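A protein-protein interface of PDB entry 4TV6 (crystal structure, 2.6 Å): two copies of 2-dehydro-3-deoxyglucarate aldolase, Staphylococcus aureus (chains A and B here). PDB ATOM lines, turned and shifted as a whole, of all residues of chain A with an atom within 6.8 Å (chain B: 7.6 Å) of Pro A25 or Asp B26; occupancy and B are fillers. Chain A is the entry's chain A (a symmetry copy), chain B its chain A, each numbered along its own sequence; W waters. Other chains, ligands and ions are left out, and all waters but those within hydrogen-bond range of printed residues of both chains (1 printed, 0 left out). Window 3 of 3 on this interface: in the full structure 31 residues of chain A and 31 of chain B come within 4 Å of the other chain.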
ATOM      1  N   ASN A  22      -2.100  -8.002 -13.820  1.00  0.00           N
ATOM      2  CA  ASN A  22      -3.502  -7.872 -13.447  1.00  0.00           C
ATOM      3  C   ASN A  22      -3.977  -6.429 -13.582  1.00  0.00           C
ATOM      4  O   ASN A  22      -3.547  -5.551 -12.833  1.00  0.00           O
ATOM      5  CB  ASN A  22      -3.718  -8.378 -12.019  1.00  0.00           C
ATOM      6  CG  ASN A  22      -5.111  -8.087 -11.499  1.00  0.00           C
ATOM      7  OD1 ASN A  22      -5.280  -7.358 -10.524  1.00  0.00           O
ATOM      8  ND2 ASN A  22      -6.119  -8.654 -12.152  1.00  0.00           N
ATOM      9  N   SER A  23      -4.862  -6.191 -14.544  1.00  0.00           N
ATOM     10  CA  SER A  23      -5.350  -4.844 -14.822  1.00  0.00           C
ATOM     11  C   SER A  23      -6.764  -4.635 -14.293  1.00  0.00           C
ATOM     12  O   SER A  23      -7.318  -3.541 -14.387  1.00  0.00           O
ATOM     13  CB  SER A  23      -5.314  -4.565 -16.325  1.00  0.00           C
ATOM     14  OG  SER A  23      -4.077  -4.963 -16.885  1.00  0.00           O
ATOM     15  N   ILE A  24      -7.346  -5.693 -13.738  1.00  0.00           N
ATOM     16  CA  ILE A  24      -8.709  -5.635 -13.233  1.00  0.00           C
ATOM     17  C   ILE A  24      -8.728  -5.911 -11.733  1.00  0.00           C
ATOM     18  O   ILE A  24      -8.588  -7.055 -11.304  1.00  0.00           O
ATOM     19  CB  ILE A  24      -9.616  -6.633 -13.971  1.00  0.00           C
ATOM     20  CG1 ILE A  24      -9.586  -6.346 -15.473  1.00  0.00           C
ATOM     21  CG2 ILE A  24     -11.038  -6.557 -13.441  1.00  0.00           C
ATOM     22  CD1 ILE A  24     -10.137  -7.459 -16.325  1.00  0.00           C
ATOM     23  N   PRO A  25      -8.906  -4.850 -10.930  1.00  0.00           N
ATOM     24  CA  PRO A  25      -8.801  -4.900  -9.469  1.00  0.00           C
ATOM     25  C   PRO A  25      -9.982  -5.594  -8.801  1.00  0.00           C
ATOM     26  O   PRO A  25     -10.600  -5.030  -7.897  1.00  0.00           O
ATOM     27  CB  PRO A  25      -8.755  -3.423  -9.078  1.00  0.00           C
ATOM     28  CG  PRO A  25      -9.559  -2.749 -10.133  1.00  0.00           C
ATOM     29  CD  PRO A  25      -9.273  -3.503 -11.407  1.00  0.00           C
ATOM     30  N   ASP A  26     -10.284  -6.810  -9.240  1.00  0.00           N
ATOM     31  CA  ASP A  26     -11.373  -7.578  -8.657  1.00  0.00           C
ATOM     32  C   ASP A  26     -10.847  -8.896  -8.097  1.00  0.00           C
ATOM     33  O   ASP A  26     -10.104  -9.605  -8.773  1.00  0.00           O
ATOM     34  CB  ASP A  26     -12.465  -7.837  -9.695  1.00  0.00           C
ATOM     35  CG  ASP A  26     -13.742  -8.362  -9.075  1.00  0.00           C
ATOM     36  OD1 ASP A  26     -13.817  -9.578  -8.803  1.00  0.00           O
ATOM     37  OD2 ASP A  26     -14.672  -7.558  -8.854  1.00  0.00           O
ATOM     38  N   PRO A  27     -11.227  -9.219  -6.850  1.00  0.00           N
ATOM     39  CA  PRO A  27     -10.766 -10.436  -6.169  1.00  0.00           C
ATOM     40  C   PRO A  27     -11.131 -11.717  -6.915  1.00  0.00           C
ATOM     41  O   PRO A  27     -10.401 -12.703  -6.814  1.00  0.00           O
ATOM     42  CB  PRO A  27     -11.477 -10.373  -4.809  1.00  0.00           C
ATOM     43  CG  PRO A  27     -12.604  -9.405  -4.997  1.00  0.00           C
ATOM     44  CD  PRO A  27     -12.112  -8.412  -5.994  1.00  0.00           C
ATOM     45  N   LEU A  28     -12.238 -11.701  -7.652  1.00  0.00           N
ATOM     46  CA  LEU A  28     -12.645 -12.865  -8.430  1.00  0.00           C
ATOM     47  C   LEU A  28     -11.683 -13.100  -9.589  1.00  0.00           C
ATOM     48  O   LEU A  28     -11.403 -14.242  -9.951  1.00  0.00           O
ATOM     49  CB  LEU A  28     -14.070 -12.699  -8.957  1.00  0.00           C
ATOM     50  CG  LEU A  28     -15.166 -12.567  -7.899  1.00  0.00           C
ATOM     51  CD1 LEU A  28     -16.506 -12.307  -8.560  1.00  0.00           C
ATOM     52  CD2 LEU A  28     -15.229 -13.815  -7.034  1.00  0.00           C
ATOM     53  N   MET A  29     -11.181 -12.013 -10.166  1.00  0.00           N
ATOM     54  CA  MET A  29     -10.199 -12.107 -11.238  1.00  0.00           C
ATOM     55  C   MET A  29      -8.902 -12.716 -10.718  1.00  0.00           C
ATOM     56  O   MET A  29      -8.258 -13.508 -11.404  1.00  0.00           O
ATOM     57  CB  MET A  29      -9.931 -10.731 -11.853  1.00  0.00           C
ATOM     58  CG  MET A  29      -8.910 -10.752 -12.976  1.00  0.00           C
ATOM     59  SD  MET A  29      -9.321 -11.932 -14.276  1.00  0.00           S
ATOM     60  CE  MET A  29     -10.941 -11.351 -14.754  1.00  0.00           C
ATOM     61  N   ILE A  30      -8.534 -12.345  -9.496  1.00  0.00           N
ATOM     62  CA  ILE A  30      -7.360 -12.907  -8.840  1.00  0.00           C
ATOM     63  C   ILE A  30      -7.519 -14.413  -8.650  1.00  0.00           C
ATOM     64  O   ILE A  30      -6.607 -15.188  -8.941  1.00  0.00           O
ATOM     65  CB  ILE A  30      -7.108 -12.245  -7.470  1.00  0.00           C
ATOM     66  CG1 ILE A  30      -6.824 -10.752  -7.642  1.00  0.00           C
ATOM     67  CG2 ILE A  30      -5.954 -12.926  -6.748  1.00  0.00           C
ATOM     68  CD1 ILE A  30      -5.551 -10.459  -8.406  1.00  0.00           C
ATOM     69  N   ILE A  43      -0.128  -7.621  -9.632  1.00  0.00           N
ATOM     70  CA  ILE A  43      -1.180  -6.629  -9.463  1.00  0.00           C
ATOM     71  C   ILE A  43      -0.667  -5.257  -9.878  1.00  0.00           C
ATOM     72  O   ILE A  43       0.098  -4.620  -9.153  1.00  0.00           O
ATOM     73  CB  ILE A  43      -1.681  -6.570  -8.012  1.00  0.00           C
ATOM     74  CG1 ILE A  43      -2.047  -7.971  -7.514  1.00  0.00           C
ATOM     75  CG2 ILE A  43      -2.871  -5.631  -7.897  1.00  0.00           C
ATOM     76  CD1 ILE A  43      -2.449  -8.012  -6.051  1.00  0.00           C
ATOM     77  N   ASP A  44      -1.093  -4.810 -11.055  1.00  0.00           N
ATOM     78  CA  ASP A  44      -0.614  -3.554 -11.617  1.00  0.00           C
ATOM     79  C   ASP A  44      -1.366  -2.361 -11.037  1.00  0.00           C
ATOM     80  O   ASP A  44      -2.525  -2.130 -11.368  1.00  0.00           O
ATOM     81  CB  ASP A  44      -0.754  -3.575 -13.138  1.00  0.00           C
ATOM     82  CG  ASP A  44       0.324  -2.772 -13.834  1.00  0.00           C
ATOM     83  OD1 ASP A  44       0.837  -1.806 -13.231  1.00  0.00           O
ATOM     84  OD2 ASP A  44       0.658  -3.110 -14.989  1.00  0.00           O
ATOM     85  N   VAL A  48      -4.024   1.255 -13.069  1.00  0.00           N
ATOM     86  CA  VAL A  48      -5.330   0.829 -12.588  1.00  0.00           C
ATOM     87  C   VAL A  48      -5.814   1.752 -11.480  1.00  0.00           C
ATOM     88  O   VAL A  48      -5.127   1.941 -10.477  1.00  0.00           O
ATOM     89  CB  VAL A  48      -5.305  -0.619 -12.060  1.00  0.00           C
ATOM     90  CG1 VAL A  48      -6.614  -0.955 -11.366  1.00  0.00           C
ATOM     91  CG2 VAL A  48      -5.030  -1.596 -13.189  1.00  0.00           C
ATOM     92  N   ALA A  49      -6.989   2.339 -11.672  1.00  0.00           N
ATOM     93  CA  ALA A  49      -7.635   3.096 -10.611  1.00  0.00           C
ATOM     94  C   ALA A  49      -8.041   2.133  -9.503  1.00  0.00           C
ATOM     95  O   ALA A  49      -9.059   1.451  -9.607  1.00  0.00           O
ATOM     96  CB  ALA A  49      -8.839   3.848 -11.141  1.00  0.00           C
ATOM     97  N   ILE A  50      -7.233   2.069  -8.451  1.00  0.00           N
ATOM     98  CA  ILE A  50      -7.466   1.098  -7.390  1.00  0.00           C
ATOM     99  C   ILE A  50      -7.277   1.705  -5.999  1.00  0.00           C
ATOM    100  O   ILE A  50      -6.235   2.285  -5.691  1.00  0.00           O
ATOM    101  CB  ILE A  50      -6.544  -0.137  -7.561  1.00  0.00           C
ATOM    102  CG1 ILE A  50      -6.698  -1.100  -6.383  1.00  0.00           C
ATOM    103  CG2 ILE A  50      -5.089   0.279  -7.738  1.00  0.00           C
ATOM    104  CD1 ILE A  50      -5.886  -2.368  -6.534  1.00  0.00           C
ATOM    105  N   ASN A  51      -8.310   1.580  -5.172  1.00  0.00           N
ATOM    106  CA  ASN A  51      -8.256   2.044  -3.792  1.00  0.00           C
ATOM    107  C   ASN A  51      -7.262   1.229  -2.979  1.00  0.00           C
ATOM    108  O   ASN A  51      -6.995   0.072  -3.299  1.00  0.00           O
ATOM    109  CB  ASN A  51      -9.642   1.972  -3.148  1.00  0.00           C
ATOM    110  CG  ASN A  51     -10.593   3.017  -3.689  1.00  0.00           C
ATOM    111  OD1 ASN A  51     -10.221   3.839  -4.526  1.00  0.00           O
ATOM    112  ND2 ASN A  51     -11.834   2.987  -3.215  1.00  0.00           N
ATOM    113  N   THR A  54      -8.796  -1.816  -1.496  1.00  0.00           N
ATOM    114  CA  THR A  54      -9.059  -2.806  -2.530  1.00  0.00           C
ATOM    115  C   THR A  54      -7.786  -3.594  -2.832  1.00  0.00           C
ATOM    116  O   THR A  54      -7.832  -4.804  -3.054  1.00  0.00           O
ATOM    117  CB  THR A  54      -9.589  -2.146  -3.822  1.00  0.00           C
ATOM    118  OG1 THR A  54     -10.785  -1.413  -3.530  1.00  0.00           O
ATOM    119  CG2 THR A  54      -9.899  -3.195  -4.881  1.00  0.00           C
ATOM    120  N   LEU A  55      -6.651  -2.903  -2.834  1.00  0.00           N
ATOM    121  CA  LEU A  55      -5.362  -3.553  -3.040  1.00  0.00           C
ATOM    122  C   LEU A  55      -5.086  -4.567  -1.935  1.00  0.00           C
ATOM    123  O   LEU A  55      -4.568  -5.653  -2.191  1.00  0.00           O
ATOM    124  CB  LEU A  55      -4.237  -2.520  -3.101  1.00  0.00           C
ATOM    125  CG  LEU A  55      -2.836  -3.091  -3.334  1.00  0.00           C
ATOM    126  CD1 LEU A  55      -2.769  -3.808  -4.674  1.00  0.00           C
ATOM    127  CD2 LEU A  55      -1.777  -2.001  -3.250  1.00  0.00           C
ATOM    128  N   LEU A  58      -7.141  -7.586  -2.567  1.00  0.00           N
ATOM    129  CA  LEU A  58      -6.585  -8.426  -3.622  1.00  0.00           C
ATOM    130  C   LEU A  58      -5.434  -9.285  -3.116  1.00  0.00           C
ATOM    131  O   LEU A  58      -5.268 -10.430  -3.535  1.00  0.00           O
ATOM    132  CB  LEU A  58      -6.113  -7.567  -4.797  1.00  0.00           C
ATOM    133  CG  LEU A  58      -7.194  -6.794  -5.553  1.00  0.00           C
ATOM    134  CD1 LEU A  58      -6.605  -6.103  -6.769  1.00  0.00           C
ATOM    135  CD2 LEU A  58      -8.329  -7.718  -5.957  1.00  0.00           C
ATOM    136  N   ASP A 237      -4.018  -9.791 -18.018  1.00  0.00           N
ATOM    137  CA  ASP A 237      -5.326 -10.437 -18.065  1.00  0.00           C
ATOM    138  C   ASP A 237      -6.286  -9.716 -19.008  1.00  0.00           C
ATOM    139  O   ASP A 237      -6.880 -10.337 -19.886  1.00  0.00           O
ATOM    140  CB  ASP A 237      -5.936 -10.532 -16.660  1.00  0.00           C
ATOM    141  CG  ASP A 237      -5.930  -9.206 -15.917  1.00  0.00           C
ATOM    142  OD1 ASP A 237      -5.647  -8.161 -16.541  1.00  0.00           O
ATOM    143  OD2 ASP A 237      -6.219  -9.214 -14.703  1.00  0.00           O
ATOM    144  N   ASN B  22     -22.222 -12.077 -16.895  1.00  0.00           N
ATOM    145  CA  ASN B  22     -21.151 -11.384 -16.193  1.00  0.00           C
ATOM    146  C   ASN B  22     -21.084 -11.812 -14.730  1.00  0.00           C
ATOM    147  O   ASN B  22     -21.987 -11.516 -13.946  1.00  0.00           O
ATOM    148  CB  ASN B  22     -21.341  -9.869 -16.302  1.00  0.00           C
ATOM    149  CG  ASN B  22     -20.377  -9.094 -15.428  1.00  0.00           C
ATOM    150  OD1 ASN B  22     -20.789  -8.379 -14.516  1.00  0.00           O
ATOM    151  ND2 ASN B  22     -19.085  -9.234 -15.699  1.00  0.00           N
ATOM    152  N   SER B  23     -20.013 -12.512 -14.372  1.00  0.00           N
ATOM    153  CA  SER B  23     -19.856 -13.036 -13.020  1.00  0.00           C
ATOM    154  C   SER B  23     -18.854 -12.222 -12.211  1.00  0.00           C
ATOM    155  O   SER B  23     -18.635 -12.484 -11.029  1.00  0.00           O
ATOM    156  CB  SER B  23     -19.416 -14.500 -13.065  1.00  0.00           C
ATOM    157  OG  SER B  23     -20.196 -15.236 -13.987  1.00  0.00           O
ATOM    158  N   ILE B  24     -18.245 -11.233 -12.855  1.00  0.00           N
ATOM    159  CA  ILE B  24     -17.236 -10.408 -12.206  1.00  0.00           C
ATOM    160  C   ILE B  24     -17.692  -8.953 -12.165  1.00  0.00           C
ATOM    161  O   ILE B  24     -17.653  -8.255 -13.177  1.00  0.00           O
ATOM    162  CB  ILE B  24     -15.881 -10.523 -12.924  1.00  0.00           C
ATOM    163  CG1 ILE B  24     -15.439 -11.987 -12.960  1.00  0.00           C
ATOM    164  CG2 ILE B  24     -14.836  -9.665 -12.232  1.00  0.00           C
ATOM    165  CD1 ILE B  24     -14.325 -12.270 -13.933  1.00  0.00           C
ATOM    166  N   PRO B  25     -18.126  -8.494 -10.980  1.00  0.00           N
ATOM    167  CA  PRO B  25     -18.741  -7.177 -10.786  1.00  0.00           C
ATOM    168  C   PRO B  25     -17.743  -6.027 -10.859  1.00  0.00           C
ATOM    169  O   PRO B  25     -17.684  -5.202  -9.946  1.00  0.00           O
ATOM    170  CB  PRO B  25     -19.339  -7.282  -9.383  1.00  0.00           C
ATOM    171  CG  PRO B  25     -18.427  -8.222  -8.676  1.00  0.00           C
ATOM    172  CD  PRO B  25     -18.003  -9.233  -9.711  1.00  0.00           C
ATOM    173  N   ASP B  26     -16.973  -5.974 -11.939  1.00  0.00           N
ATOM    174  CA  ASP B  26     -16.006  -4.905 -12.128  1.00  0.00           C
ATOM    175  C   ASP B  26     -16.308  -4.142 -13.414  1.00  0.00           C
ATOM    176  O   ASP B  26     -16.521  -4.751 -14.462  1.00  0.00           O
ATOM    177  CB  ASP B  26     -14.584  -5.465 -12.161  1.00  0.00           C
ATOM    178  CG  ASP B  26     -13.530  -4.383 -12.054  1.00  0.00           C
ATOM    179  OD1 ASP B  26     -13.223  -3.745 -13.082  1.00  0.00           O
ATOM    180  OD2 ASP B  26     -13.013  -4.165 -10.938  1.00  0.00           O
ATOM    181  N   PRO B  27     -16.337  -2.802 -13.332  1.00  0.00           N
ATOM    182  CA  PRO B  27     -16.654  -1.942 -14.479  1.00  0.00           C
ATOM    183  C   PRO B  27     -15.698  -2.130 -15.655  1.00  0.00           C
ATOM    184  O   PRO B  27     -16.107  -1.944 -16.800  1.00  0.00           O
ATOM    185  CB  PRO B  27     -16.540  -0.523 -13.902  1.00  0.00           C
ATOM    186  CG  PRO B  27     -15.742  -0.672 -12.644  1.00  0.00           C
ATOM    187  CD  PRO B  27     -16.092  -2.019 -12.109  1.00  0.00           C
ATOM    188  N   LEU B  28     -14.450  -2.496 -15.374  1.00  0.00           N
ATOM    189  CA  LEU B  28     -13.478  -2.738 -16.434  1.00  0.00           C
ATOM    190  C   LEU B  28     -13.841  -3.991 -17.221  1.00  0.00           C
ATOM    191  O   LEU B  28     -13.637  -4.053 -18.433  1.00  0.00           O
ATOM    192  CB  LEU B  28     -12.067  -2.868 -15.861  1.00  0.00           C
ATOM    193  CG  LEU B  28     -11.519  -1.638 -15.138  1.00  0.00           C
ATOM    194  CD1 LEU B  28     -10.161  -1.943 -14.535  1.00  0.00           C
ATOM    195  CD2 LEU B  28     -11.431  -0.453 -16.086  1.00  0.00           C
ATOM    196  N   MET B  29     -14.380  -4.988 -16.525  1.00  0.00           N
ATOM    197  CA  MET B  29     -14.832  -6.211 -17.175  1.00  0.00           C
ATOM    198  C   MET B  29     -16.002  -5.916 -18.106  1.00  0.00           C
ATOM    199  O   MET B  29     -16.100  -6.481 -19.194  1.00  0.00           O
ATOM    200  CB  MET B  29     -15.229  -7.263 -16.137  1.00  0.00           C
ATOM    201  CG  MET B  29     -15.718  -8.566 -16.744  1.00  0.00           C
ATOM    202  SD  MET B  29     -14.547  -9.277 -17.916  1.00  0.00           S
ATOM    203  CE  MET B  29     -13.097  -9.434 -16.884  1.00  0.00           C
ATOM    204  N   ILE B  30     -16.880  -5.019 -17.670  1.00  0.00           N
ATOM    205  CA  ILE B  30     -18.005  -4.579 -18.487  1.00  0.00           C
ATOM    206  C   ILE B  30     -17.511  -3.906 -19.764  1.00  0.00           C
ATOM    207  O   ILE B  30     -17.996  -4.191 -20.859  1.00  0.00           O
ATOM    208  CB  ILE B  30     -18.916  -3.603 -17.715  1.00  0.00           C
ATOM    209  CG1 ILE B  30     -19.524  -4.293 -16.492  1.00  0.00           C
ATOM    210  CG2 ILE B  30     -20.013  -3.063 -18.621  1.00  0.00           C
ATOM    211  CD1 ILE B  30     -20.455  -5.434 -16.838  1.00  0.00           C
ATOM    212  N   GLU B  31     -16.534  -3.020 -19.612  1.00  0.00           N
ATOM    213  CA  GLU B  31     -15.978  -2.286 -20.743  1.00  0.00           C
ATOM    214  C   GLU B  31     -15.197  -3.211 -21.674  1.00  0.00           C
ATOM    215  O   GLU B  31     -15.122  -2.972 -22.879  1.00  0.00           O
ATOM    216  CB  GLU B  31     -15.089  -1.145 -20.242  1.00  0.00           C
ATOM    217  CG  GLU B  31     -15.866  -0.027 -19.558  1.00  0.00           C
ATOM    218  CD  GLU B  31     -14.996   0.847 -18.670  1.00  0.00           C
ATOM    219  OE1 GLU B  31     -13.820   0.495 -18.446  1.00  0.00           O
ATOM    220  OE2 GLU B  31     -15.493   1.889 -18.193  1.00  0.00           O
ATOM    221  N   VAL B  32     -14.627  -4.269 -21.109  1.00  0.00           N
ATOM    222  CA  VAL B  32     -13.916  -5.273 -21.897  1.00  0.00           C
ATOM    223  C   VAL B  32     -14.898  -6.068 -22.756  1.00  0.00           C
ATOM    224  O   VAL B  32     -14.639  -6.332 -23.933  1.00  0.00           O
ATOM    225  CB  VAL B  32     -13.109  -6.231 -20.989  1.00  0.00           C
ATOM    226  CG1 VAL B  32     -12.889  -7.581 -21.662  1.00  0.00           C
ATOM    227  CG2 VAL B  32     -11.783  -5.600 -20.600  1.00  0.00           C
ATOM    228  N   ILE B  33     -16.027  -6.437 -22.160  1.00  0.00           N
ATOM    229  CA  ILE B  33     -17.077  -7.158 -22.871  1.00  0.00           C
ATOM    230  C   ILE B  33     -17.631  -6.322 -24.026  1.00  0.00           C
ATOM    231  O   ILE B  33     -17.806  -6.821 -25.138  1.00  0.00           O
ATOM    232  CB  ILE B  33     -18.225  -7.556 -21.920  1.00  0.00           C
ATOM    233  CG1 ILE B  33     -17.733  -8.585 -20.898  1.00  0.00           C
ATOM    234  CG2 ILE B  33     -19.397  -8.123 -22.700  1.00  0.00           C
ATOM    235  CD1 ILE B  33     -18.676  -8.801 -19.738  1.00  0.00           C
ATOM    236  N   VAL B  48     -23.385 -13.661  -7.617  1.00  0.00           N
ATOM    237  CA  VAL B  48     -22.283 -12.729  -7.435  1.00  0.00           C
ATOM    238  C   VAL B  48     -22.519 -11.863  -6.206  1.00  0.00           C
ATOM    239  O   VAL B  48     -23.548 -11.200  -6.094  1.00  0.00           O
ATOM    240  CB  VAL B  48     -22.093 -11.815  -8.662  1.00  0.00           C
ATOM    241  CG1 VAL B  48     -21.091 -10.715  -8.356  1.00  0.00           C
ATOM    242  CG2 VAL B  48     -21.649 -12.625  -9.868  1.00  0.00           C
ATOM    243  N   ILE B  50     -22.458  -8.803  -4.820  1.00  0.00           N
ATOM    244  CA  ILE B  50     -22.368  -7.477  -5.417  1.00  0.00           C
ATOM    245  C   ILE B  50     -23.216  -6.448  -4.669  1.00  0.00           C
ATOM    246  O   ILE B  50     -24.416  -6.635  -4.463  1.00  0.00           O
ATOM    247  CB  ILE B  50     -22.777  -7.516  -6.912  1.00  0.00           C
ATOM    248  CG1 ILE B  50     -22.803  -6.108  -7.509  1.00  0.00           C
ATOM    249  CG2 ILE B  50     -24.120  -8.212  -7.100  1.00  0.00           C
ATOM    250  CD1 ILE B  50     -23.112  -6.089  -8.990  1.00  0.00           C
ATOM    251  N   THR B  54     -22.532  -0.853  -6.461  1.00  0.00           N
ATOM    252  CA  THR B  54     -21.641  -1.421  -7.463  1.00  0.00           C
ATOM    253  C   THR B  54     -22.439  -1.813  -8.705  1.00  0.00           C
ATOM    254  O   THR B  54     -21.978  -1.635  -9.832  1.00  0.00           O
ATOM    255  CB  THR B  54     -20.882  -2.648  -6.914  1.00  0.00           C
ATOM    256  OG1 THR B  54     -20.134  -2.270  -5.752  1.00  0.00           O
ATOM    257  CG2 THR B  54     -19.925  -3.208  -7.958  1.00  0.00           C
ATOM    258  N   HIS B  57     -23.015   1.151 -10.587  1.00  0.00           N
ATOM    259  CA  HIS B  57     -21.755   1.498 -11.233  1.00  0.00           C
ATOM    260  C   HIS B  57     -21.608   0.732 -12.545  1.00  0.00           C
ATOM    261  O   HIS B  57     -21.167   1.287 -13.552  1.00  0.00           O
ATOM    262  CB  HIS B  57     -20.579   1.196 -10.300  1.00  0.00           C
ATOM    263  CG  HIS B  57     -19.279   1.801 -10.723  1.00  0.00           C
ATOM    264  ND1 HIS B  57     -19.042   2.239 -12.015  1.00  0.00           N
ATOM    265  CD2 HIS B  57     -18.137   2.043 -10.036  1.00  0.00           C
ATOM    266  CE1 HIS B  57     -17.812   2.723 -12.092  1.00  0.00           C
ATOM    267  NE2 HIS B  57     -17.246   2.613 -10.906  1.00  0.00           N
ATOM    268  N   LEU B  58     -21.989  -0.542 -12.526  1.00  0.00           N
ATOM    269  CA  LEU B  58     -21.860  -1.404 -13.696  1.00  0.00           C
ATOM    270  C   LEU B  58     -22.827  -1.005 -14.803  1.00  0.00           C
ATOM    271  O   LEU B  58     -22.499  -1.086 -15.987  1.00  0.00           O
ATOM    272  CB  LEU B  58     -22.090  -2.866 -13.310  1.00  0.00           C
ATOM    273  CG  LEU B  58     -21.070  -3.487 -12.354  1.00  0.00           C
ATOM    274  CD1 LEU B  58     -21.341  -4.969 -12.173  1.00  0.00           C
ATOM    275  CD2 LEU B  58     -19.656  -3.256 -12.857  1.00  0.00           C
ATOM    276  N   ALA B  61     -21.471   2.004 -16.394  1.00  0.00           N
ATOM    277  CA  ALA B  61     -20.317   1.603 -17.191  1.00  0.00           C
ATOM    278  C   ALA B  61     -20.748   0.976 -18.512  1.00  0.00           C
ATOM    279  O   ALA B  61     -20.115   1.189 -19.547  1.00  0.00           O
ATOM    280  CB  ALA B  61     -19.443   0.639 -16.408  1.00  0.00           C
ATOM    281  N   ASP B 237     -18.480 -14.820 -18.622  1.00  0.00           N
ATOM    282  CA  ASP B 237     -17.121 -14.300 -18.739  1.00  0.00           C
ATOM    283  C   ASP B 237     -16.127 -15.110 -17.911  1.00  0.00           C
ATOM    284  O   ASP B 237     -15.104 -15.554 -18.427  1.00  0.00           O
ATOM    285  CB  ASP B 237     -17.069 -12.821 -18.336  1.00  0.00           C
ATOM    286  CG  ASP B 237     -17.718 -12.549 -16.989  1.00  0.00           C
ATOM    287  OD1 ASP B 237     -18.033 -13.513 -16.259  1.00  0.00           O
ATOM    288  OD2 ASP B 237     -17.904 -11.359 -16.659  1.00  0.00           O
HETATM  289  O   HOH W   1     -14.163  -5.064  -8.854  1.00  0.00           O
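Of the printed residues of chain B, Ile A24 touches Asp B26 and Met B29. Of the printed residues of chain B, Asp A26 touches Ile B24 (3.6 Å), Pro B25 (3.8 Å) and Asp B26 (3.9 Å). Ile A50 touches none of the printed residues of chain B. Printed residues of chain A within 4 Å of Ile B24: Asp A26 (3.6 Å) and Met A29 (3.6 Å). Asp B26 touches three residues of chain A. Leu B58 touches none of the printed residues of chain A. The nearest residue of chain B that does not touch Pro A25 is Pro B27 (6.9 Å). The nearest residue of chain A that does not touch Asp B26 is Ser A23 (6.1 Å). The nearest printed residue of chain B that does not touch Asp A26 is Ser B23 (6.1 Å).
The side-chain amide nitrogen (ND2) of Asn B22 sits at hydrogen-bond distance from the backbone carbonyl oxygen (O) of Ile B24 (3.1 Å). The backbone NH (N) of Ser B23 lies within hydrogen-bond range of the side-chain carboxylate (OD1) of Asp B237, 2.9 Å away. The side-chain carboxylate of Asp B26 sits at hydrogen-bond distance from the backbone NH of Leu B28. The side-chain amide nitrogen (ND2) of Asn A22 is in hydrogen-bond range of the backbone carbonyl oxygen (O) of Ile A24 (3.1 Å). The backbone NH of Ser A23 sits at hydrogen-bond distance from the side-chain carboxylate of Asp A237, 2.9 Å away. OD1 of Asp A26 sits at hydrogen-bond distance from N of Leu A28 (2.9 Å).
Water W1 bridges the side-chain carboxylate (OD2) of Asp B26 (2.5 Å) and the side-chain carboxylate (OD2) of Asp A26 (2.5 Å).
Ile A24 touches Asp B26, and with the chains exchanged Asp A26 touches Ile B24. Ile A24 touches Met B29, and with the chains exchanged Met A29 touches Ile B24. Pro A25 touches Asp B26, and with the chains exchanged Asp A26 touches Pro B25. Met A29 touches its own counterpart, Met B29. Of the 12 pairs that touch across the chains among the printed residues, 12 have their exchanged pair printed and touching as well.
O of Ser A23 touches CD1 of Leu B28, at 3.3 Å. Ile A24 touches Asp B26. Asp B26 touches Pro A25 (OD2 to CG, 3.8 Å). Pro A25 touches Leu B28. Ile B24 touches Asp A26. CG of Pro B25 touches OD2 of Asp A26 (3.8 Å). OD2 of Asp A26 touches CB of Asp B26, 3.9 Å away. O of Ser B23 touches CD1 of Leu A28 (3.3 Å). CE of Met A29 touches CD1 of Ile B24, at 3.6 Å. Met A29 touches Met B29 (CE to CE, 3.6 Å).
Of the 19 printed residues of chain A, 6 touch a printed residue of chain B. Among the printed residues, no Asp or Glu carboxylate lies within 4 Å of a Lys or Arg side-chain nitrogen of the other chain.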
